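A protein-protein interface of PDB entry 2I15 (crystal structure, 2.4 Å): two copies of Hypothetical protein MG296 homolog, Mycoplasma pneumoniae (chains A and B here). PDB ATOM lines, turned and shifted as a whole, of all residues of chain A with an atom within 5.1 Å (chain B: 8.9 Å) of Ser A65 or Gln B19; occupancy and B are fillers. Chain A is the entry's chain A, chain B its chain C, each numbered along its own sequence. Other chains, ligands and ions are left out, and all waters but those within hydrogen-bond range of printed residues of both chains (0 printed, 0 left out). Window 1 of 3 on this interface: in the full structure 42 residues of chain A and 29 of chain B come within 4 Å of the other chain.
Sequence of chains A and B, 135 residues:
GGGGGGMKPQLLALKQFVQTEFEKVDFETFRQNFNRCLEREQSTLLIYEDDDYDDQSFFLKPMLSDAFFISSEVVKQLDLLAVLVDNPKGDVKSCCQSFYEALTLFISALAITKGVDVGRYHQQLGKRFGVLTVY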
ATOM      1  N   LYS A  61     -23.753 -14.795 -12.515  1.00  0.00           N
ATOM      2  CA  LYS A  61     -22.398 -14.928 -11.987  1.00  0.00           C
ATOM      3  C   LYS A  61     -21.881 -13.685 -11.242  1.00  0.00           C
ATOM      4  O   LYS A  61     -21.176 -13.805 -10.242  1.00  0.00           O
ATOM      5  CB  LYS A  61     -21.482 -15.285 -13.142  1.00  0.00           C
ATOM      6  CG  LYS A  61     -20.043 -15.593 -12.803  1.00  0.00           C
ATOM      7  CD  LYS A  61     -19.320 -16.140 -14.042  1.00  0.00           C
ATOM      8  CE  LYS A  61     -19.879 -15.534 -15.351  1.00  0.00           C
ATOM      9  NZ  LYS A  61     -19.867 -14.038 -15.345  1.00  0.00           N
ATOM     10  N   PRO A  62     -22.201 -12.480 -11.730  1.00  0.00           N
ATOM     11  CA  PRO A  62     -21.792 -11.213 -11.126  1.00  0.00           C
ATOM     12  C   PRO A  62     -22.670 -10.877  -9.942  1.00  0.00           C
ATOM     13  O   PRO A  62     -22.185 -10.384  -8.931  1.00  0.00           O
ATOM     14  CB  PRO A  62     -21.940 -10.231 -12.283  1.00  0.00           C
ATOM     15  CG  PRO A  62     -21.582 -11.071 -13.429  1.00  0.00           C
ATOM     16  CD  PRO A  62     -22.478 -12.256 -13.148  1.00  0.00           C
ATOM     17  N   MET A  63     -23.966 -11.144 -10.087  1.00  0.00           N
ATOM     18  CA  MET A  63     -24.935 -10.910  -9.019  1.00  0.00           C
ATOM     19  C   MET A  63     -24.497 -11.759  -7.826  1.00  0.00           C
ATOM     20  O   MET A  63     -24.655 -11.374  -6.676  1.00  0.00           O
ATOM     21  CB  MET A  63     -26.324 -11.340  -9.474  1.00  0.00           C
ATOM     22  CG  MET A  63     -27.197 -10.183  -9.808  1.00  0.00           C
ATOM     23  SD  MET A  63     -27.210  -9.001  -8.454  1.00  0.00           S
ATOM     24  CE  MET A  63     -28.864  -9.295  -7.770  1.00  0.00           C
ATOM     25  N   LEU A  64     -23.955 -12.929  -8.135  1.00  0.00           N
ATOM     26  CA  LEU A  64     -23.443 -13.861  -7.148  1.00  0.00           C
ATOM     27  C   LEU A  64     -22.397 -13.139  -6.287  1.00  0.00           C
ATOM     28  O   LEU A  64     -22.597 -12.932  -5.088  1.00  0.00           O
ATOM     29  CB  LEU A  64     -22.796 -15.029  -7.882  1.00  0.00           C
ATOM     30  CG  LEU A  64     -23.164 -16.435  -7.458  1.00  0.00           C
ATOM     31  CD1 LEU A  64     -22.469 -16.752  -6.146  1.00  0.00           C
ATOM     32  CD2 LEU A  64     -24.682 -16.535  -7.346  1.00  0.00           C
ATOM     33  N   SER A  65     -21.281 -12.759  -6.906  1.00  0.00           N
ATOM     34  CA  SER A  65     -20.238 -12.051  -6.182  1.00  0.00           C
ATOM     35  C   SER A  65     -20.818 -10.764  -5.585  1.00  0.00           C
ATOM     36  O   SER A  65     -20.498 -10.383  -4.466  1.00  0.00           O
ATOM     37  CB  SER A  65     -19.072 -11.707  -7.116  1.00  0.00           C
ATOM     38  OG  SER A  65     -18.481 -12.881  -7.657  1.00  0.00           O
ATOM     39  N   ASP A  66     -21.686 -10.105  -6.335  1.00  0.00           N
ATOM     40  CA  ASP A  66     -22.305  -8.865  -5.876  1.00  0.00           C
ATOM     41  C   ASP A  66     -22.957  -9.076  -4.508  1.00  0.00           C
ATOM     42  O   ASP A  66     -22.505  -8.518  -3.491  1.00  0.00           O
ATOM     43  CB  ASP A  66     -23.362  -8.397  -6.883  1.00  0.00           C
ATOM     44  CG  ASP A  66     -23.004  -7.083  -7.527  1.00  0.00           C
ATOM     45  OD1 ASP A  66     -22.899  -6.079  -6.788  1.00  0.00           O
ATOM     46  OD2 ASP A  66     -22.822  -7.037  -8.768  1.00  0.00           O
ATOM     47  N   ALA A  67     -24.002  -9.908  -4.504  1.00  0.00           N
ATOM     48  CA  ALA A  67     -24.806 -10.252  -3.323  1.00  0.00           C
ATOM     49  C   ALA A  67     -24.036 -10.863  -2.141  1.00  0.00           C
ATOM     50  O   ALA A  67     -24.526 -10.836  -1.024  1.00  0.00           O
ATOM     51  CB  ALA A  67     -25.948 -11.182  -3.742  1.00  0.00           C
ATOM     52  N   PHE A  68     -22.856 -11.434  -2.398  1.00  0.00           N
ATOM     53  CA  PHE A  68     -21.999 -11.999  -1.339  1.00  0.00           C
ATOM     54  C   PHE A  68     -21.402 -10.844  -0.572  1.00  0.00           C
ATOM     55  O   PHE A  68     -21.372 -10.838   0.660  1.00  0.00           O
ATOM     56  CB  PHE A  68     -20.837 -12.809  -1.922  1.00  0.00           C
ATOM     57  CG  PHE A  68     -21.147 -14.257  -2.161  1.00  0.00           C
ATOM     58  CD1 PHE A  68     -20.417 -14.979  -3.102  1.00  0.00           C
ATOM     59  CD2 PHE A  68     -22.160 -14.901  -1.458  1.00  0.00           C
ATOM     60  CE1 PHE A  68     -20.699 -16.321  -3.341  1.00  0.00           C
ATOM     61  CE2 PHE A  68     -22.448 -16.238  -1.690  1.00  0.00           C
ATOM     62  CZ  PHE A  68     -21.717 -16.950  -2.636  1.00  0.00           C
ATOM     63  N   PHE A  69     -20.916  -9.865  -1.326  1.00  0.00           N
ATOM     64  CA  PHE A  69     -20.324  -8.677  -0.744  1.00  0.00           C
ATOM     65  C   PHE A  69     -21.370  -8.017   0.124  1.00  0.00           C
ATOM     66  O   PHE A  69     -21.073  -7.547   1.222  1.00  0.00           O
ATOM     67  CB  PHE A  69     -19.875  -7.724  -1.845  1.00  0.00           C
ATOM     68  CG  PHE A  69     -18.603  -8.134  -2.514  1.00  0.00           C
ATOM     69  CD1 PHE A  69     -17.980  -7.280  -3.419  1.00  0.00           C
ATOM     70  CD2 PHE A  69     -18.003  -9.357  -2.218  1.00  0.00           C
ATOM     71  CE1 PHE A  69     -16.771  -7.634  -4.021  1.00  0.00           C
ATOM     72  CE2 PHE A  69     -16.796  -9.725  -2.815  1.00  0.00           C
ATOM     73  CZ  PHE A  69     -16.176  -8.861  -3.718  1.00  0.00           C
ATOM     74  N   LEU B  11     -15.088 -13.429   8.743  1.00  0.00           N
ATOM     75  CA  LEU B  11     -16.199 -13.212   7.828  1.00  0.00           C
ATOM     76  C   LEU B  11     -15.625 -13.218   6.435  1.00  0.00           C
ATOM     77  O   LEU B  11     -15.988 -14.049   5.596  1.00  0.00           O
ATOM     78  CB  LEU B  11     -16.876 -11.868   8.104  1.00  0.00           C
ATOM     79  CG  LEU B  11     -18.408 -11.828   8.182  1.00  0.00           C
ATOM     80  CD1 LEU B  11     -18.924 -10.634   7.403  1.00  0.00           C
ATOM     81  CD2 LEU B  11     -19.021 -13.108   7.638  1.00  0.00           C
ATOM     82  N   LEU B  12     -14.704 -12.291   6.208  1.00  0.00           N
ATOM     83  CA  LEU B  12     -14.037 -12.138   4.924  1.00  0.00           C
ATOM     84  C   LEU B  12     -13.542 -13.461   4.334  1.00  0.00           C
ATOM     85  O   LEU B  12     -13.798 -13.757   3.170  1.00  0.00           O
ATOM     86  CB  LEU B  12     -12.858 -11.166   5.074  1.00  0.00           C
ATOM     87  CG  LEU B  12     -12.283 -10.568   3.792  1.00  0.00           C
ATOM     88  CD1 LEU B  12     -13.376  -9.805   3.053  1.00  0.00           C
ATOM     89  CD2 LEU B  12     -11.130  -9.646   4.141  1.00  0.00           C
ATOM     90  N   ALA B  13     -12.838 -14.258   5.132  1.00  0.00           N
ATOM     91  CA  ALA B  13     -12.304 -15.537   4.648  1.00  0.00           C
ATOM     92  C   ALA B  13     -13.377 -16.550   4.255  1.00  0.00           C
ATOM     93  O   ALA B  13     -13.161 -17.397   3.382  1.00  0.00           O
ATOM     94  CB  ALA B  13     -11.377 -16.152   5.687  1.00  0.00           C
ATOM     95  N   LEU B  14     -14.530 -16.460   4.911  1.00  0.00           N
ATOM     96  CA  LEU B  14     -15.643 -17.363   4.647  1.00  0.00           C
ATOM     97  C   LEU B  14     -16.295 -16.936   3.333  1.00  0.00           C
ATOM     98  O   LEU B  14     -16.637 -17.774   2.488  1.00  0.00           O
ATOM     99  CB  LEU B  14     -16.653 -17.289   5.797  1.00  0.00           C
ATOM    100  CG  LEU B  14     -17.688 -18.389   6.038  1.00  0.00           C
ATOM    101  CD1 LEU B  14     -18.842 -17.767   6.784  1.00  0.00           C
ATOM    102  CD2 LEU B  14     -18.180 -18.997   4.755  1.00  0.00           C
ATOM    103  N   LYS B  15     -16.455 -15.622   3.166  1.00  0.00           N
ATOM    104  CA  LYS B  15     -17.041 -15.067   1.946  1.00  0.00           C
ATOM    105  C   LYS B  15     -16.085 -15.366   0.813  1.00  0.00           C
ATOM    106  O   LYS B  15     -16.484 -15.734  -0.301  1.00  0.00           O
ATOM    107  CB  LYS B  15     -17.216 -13.546   2.058  1.00  0.00           C
ATOM    108  CG  LYS B  15     -17.765 -12.910   0.795  1.00  0.00           C
ATOM    109  CD  LYS B  15     -17.944 -11.425   0.959  1.00  0.00           C
ATOM    110  CE  LYS B  15     -16.617 -10.703   1.163  1.00  0.00           C
ATOM    111  NZ  LYS B  15     -16.138 -10.036  -0.086  1.00  0.00           N
ATOM    112  N   GLN B  16     -14.810 -15.167   1.117  1.00  0.00           N
ATOM    113  CA  GLN B  16     -13.736 -15.410   0.176  1.00  0.00           C
ATOM    114  C   GLN B  16     -13.940 -16.815  -0.361  1.00  0.00           C
ATOM    115  O   GLN B  16     -13.993 -17.051  -1.573  1.00  0.00           O
ATOM    116  CB  GLN B  16     -12.405 -15.350   0.911  1.00  0.00           C
ATOM    117  CG  GLN B  16     -11.335 -14.592   0.177  1.00  0.00           C
ATOM    118  CD  GLN B  16     -11.744 -13.170  -0.080  1.00  0.00           C
ATOM    119  OE1 GLN B  16     -12.632 -12.907  -0.890  1.00  0.00           O
ATOM    120  NE2 GLN B  16     -11.112 -12.237   0.623  1.00  0.00           N
ATOM    121  N   PHE B  17     -14.062 -17.736   0.583  1.00  0.00           N
ATOM    122  CA  PHE B  17     -14.246 -19.151   0.318  1.00  0.00           C
ATOM    123  C   PHE B  17     -15.450 -19.506  -0.568  1.00  0.00           C
ATOM    124  O   PHE B  17     -15.280 -20.067  -1.647  1.00  0.00           O
ATOM    125  CB  PHE B  17     -14.344 -19.888   1.658  1.00  0.00           C
ATOM    126  CG  PHE B  17     -14.464 -21.367   1.524  1.00  0.00           C
ATOM    127  CD1 PHE B  17     -13.413 -22.116   1.008  1.00  0.00           C
ATOM    128  CD2 PHE B  17     -15.647 -22.011   1.871  1.00  0.00           C
ATOM    129  CE1 PHE B  17     -13.544 -23.485   0.836  1.00  0.00           C
ATOM    130  CE2 PHE B  17     -15.781 -23.375   1.701  1.00  0.00           C
ATOM    131  CZ  PHE B  17     -14.732 -24.114   1.182  1.00  0.00           C
ATOM    132  N   VAL B  18     -16.664 -19.188  -0.125  1.00  0.00           N
ATOM    133  CA  VAL B  18     -17.849 -19.534  -0.913  1.00  0.00           C
ATOM    134  C   VAL B  18     -17.799 -18.906  -2.296  1.00  0.00           C
ATOM    135  O   VAL B  18     -18.284 -19.491  -3.271  1.00  0.00           O
ATOM    136  CB  VAL B  18     -19.186 -19.121  -0.215  1.00  0.00           C
ATOM    137  CG1 VAL B  18     -19.121 -19.447   1.266  1.00  0.00           C
ATOM    138  CG2 VAL B  18     -19.471 -17.659  -0.426  1.00  0.00           C
ATOM    139  N   GLN B  19     -17.209 -17.713  -2.372  1.00  0.00           N
ATOM    140  CA  GLN B  19     -17.071 -17.001  -3.644  1.00  0.00           C
ATOM    141  C   GLN B  19     -16.073 -17.734  -4.539  1.00  0.00           C
ATOM    142  O   GLN B  19     -16.376 -18.093  -5.683  1.00  0.00           O
ATOM    143  CB  GLN B  19     -16.567 -15.577  -3.417  1.00  0.00           C
ATOM    144  CG  GLN B  19     -16.393 -14.822  -4.696  1.00  0.00           C
ATOM    145  CD  GLN B  19     -16.139 -13.358  -4.461  1.00  0.00           C
ATOM    146  OE1 GLN B  19     -16.608 -12.784  -3.471  1.00  0.00           O
ATOM    147  NE2 GLN B  19     -15.404 -12.731  -5.377  1.00  0.00           N
ATOM    148  N   THR B  20     -14.885 -17.961  -3.992  1.00  0.00           N
ATOM    149  CA  THR B  20     -13.827 -18.639  -4.716  1.00  0.00           C
ATOM    150  C   THR B  20     -14.267 -20.018  -5.172  1.00  0.00           C
ATOM    151  O   THR B  20     -13.932 -20.439  -6.282  1.00  0.00           O
ATOM    152  CB  THR B  20     -12.567 -18.771  -3.855  1.00  0.00           C
ATOM    153  OG1 THR B  20     -12.024 -17.468  -3.606  1.00  0.00           O
ATOM    154  CG2 THR B  20     -11.530 -19.603  -4.589  1.00  0.00           C
ATOM    155  N   GLU B  21     -15.012 -20.718  -4.316  1.00  0.00           N
ATOM    156  CA  GLU B  21     -15.503 -22.057  -4.646  1.00  0.00           C
ATOM    157  C   GLU B  21     -16.596 -22.002  -5.721  1.00  0.00           C
ATOM    158  O   GLU B  21     -16.802 -22.972  -6.466  1.00  0.00           O
ATOM    159  CB  GLU B  21     -16.045 -22.761  -3.398  1.00  0.00           C
ATOM    160  CG  GLU B  21     -16.043 -24.282  -3.515  1.00  0.00           C
ATOM    161  CD  GLU B  21     -14.930 -24.922  -2.715  1.00  0.00           C
ATOM    162  OE1 GLU B  21     -13.814 -24.368  -2.703  1.00  0.00           O
ATOM    163  OE2 GLU B  21     -15.169 -25.980  -2.102  1.00  0.00           O
ATOM    164  N   PHE B  22     -17.307 -20.882  -5.798  1.00  0.00           N
ATOM    165  CA  PHE B  22     -18.343 -20.737  -6.807  1.00  0.00           C
ATOM    166  C   PHE B  22     -17.678 -20.441  -8.150  1.00  0.00           C
ATOM    167  O   PHE B  22     -18.175 -20.829  -9.212  1.00  0.00           O
ATOM    168  CB  PHE B  22     -19.275 -19.578  -6.467  1.00  0.00           C
ATOM    169  CG  PHE B  22     -20.065 -19.083  -7.652  1.00  0.00           C
ATOM    170  CD1 PHE B  22     -21.159 -19.796  -8.124  1.00  0.00           C
ATOM    171  CD2 PHE B  22     -19.675 -17.934  -8.331  1.00  0.00           C
ATOM    172  CE1 PHE B  22     -21.850 -19.372  -9.254  1.00  0.00           C
ATOM    173  CE2 PHE B  22     -20.356 -17.506  -9.458  1.00  0.00           C
ATOM    174  CZ  PHE B  22     -21.448 -18.227  -9.922  1.00  0.00           C
ATOM    175  N   GLU B  23     -16.550 -19.746  -8.089  1.00  0.00           N
ATOM    176  CA  GLU B  23     -15.831 -19.369  -9.293  1.00  0.00           C
ATOM    177  C   GLU B  23     -15.158 -20.542  -9.990  1.00  0.00           C
ATOM    178  O   GLU B  23     -15.179 -20.618 -11.218  1.00  0.00           O
ATOM    179  CB  GLU B  23     -14.789 -18.300  -8.967  1.00  0.00           C
ATOM    180  CG  GLU B  23     -15.369 -17.025  -8.383  1.00  0.00           C
ATOM    181  CD  GLU B  23     -14.295 -16.021  -8.030  1.00  0.00           C
ATOM    182  OE1 GLU B  23     -13.213 -16.465  -7.593  1.00  0.00           O
ATOM    183  OE2 GLU B  23     -14.525 -14.795  -8.173  1.00  0.00           O
ATOM    184  N   LYS B  24     -14.567 -21.457  -9.220  1.00  0.00           N
ATOM    185  CA  LYS B  24     -13.879 -22.615  -9.808  1.00  0.00           C
ATOM    186  C   LYS B  24     -14.787 -23.804 -10.065  1.00  0.00           C
ATOM    187  O   LYS B  24     -14.357 -24.949  -9.971  1.00  0.00           O
ATOM    188  CB  LYS B  24     -12.710 -23.057  -8.923  1.00  0.00           C
ATOM    189  CG  LYS B  24     -13.091 -23.510  -7.530  1.00  0.00           C
ATOM    190  CD  LYS B  24     -11.953 -23.181  -6.556  1.00  0.00           C
ATOM    191  CE  LYS B  24     -11.994 -24.022  -5.280  1.00  0.00           C
ATOM    192  NZ  LYS B  24     -13.119 -25.002  -5.215  1.00  0.00           N
ATOM    193  N   VAL B  25     -16.045 -23.540 -10.396  1.00  0.00           N
ATOM    194  CA  VAL B  25     -16.989 -24.621 -10.644  1.00  0.00           C
ATOM    195  C   VAL B  25     -17.729 -24.285 -11.938  1.00  0.00           C
ATOM    196  O   VAL B  25     -17.879 -23.108 -12.275  1.00  0.00           O
ATOM    197  CB  VAL B  25     -17.992 -24.757  -9.442  1.00  0.00           C
ATOM    198  CG1 VAL B  25     -19.244 -23.901  -9.679  1.00  0.00           C
ATOM    199  CG2 VAL B  25     -18.349 -26.210  -9.222  1.00  0.00           C
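CE2 of Phe B22 touches CG of Lys A61, at 3.9 Å.
CG of Leu A64 touches CZ of Phe B22 (3.5 Å).
Ser A65 touches Gln B19 (OG to NE2, 3.8 Å).
O of Phe A68 touches CD of Lys B15 (3.5 Å).
Val B18 touches Phe A68.
Phe A68 touches Gln B19 (CE1 to CA, 3.7 Å).
Lys B15 touches Phe A69.
Phe A69 touches Gln B19.
Of the 15 printed residues of chain B, 4 touch a printed residue of chain A.
Among the printed residues, no Asp or Glu carboxylate lies within 4 Å of a Lys or Arg side-chain nitrogen of the other chain.
Ser A65 touches one residue of chain B.
Of the printed residues of chain A, Val B18 touches Phe A68.
Of the printed residues of chain B, Leu A64 touches Phe B22.
Printed residues of chain B within 4 Å of Phe A69: Lys B15 (2.8 Å) and Gln B19 (3.1 Å).
Gln B16 touches none of the printed residues of chain A.
The nearest printed residue of chain B that does not touch Phe A68 is Phe B22 (4.7 Å).
No position is printed for both chains.
Of the 8 pairs that touch across the chains among the printed residues, none has its exchanged pair printed and touching as well.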
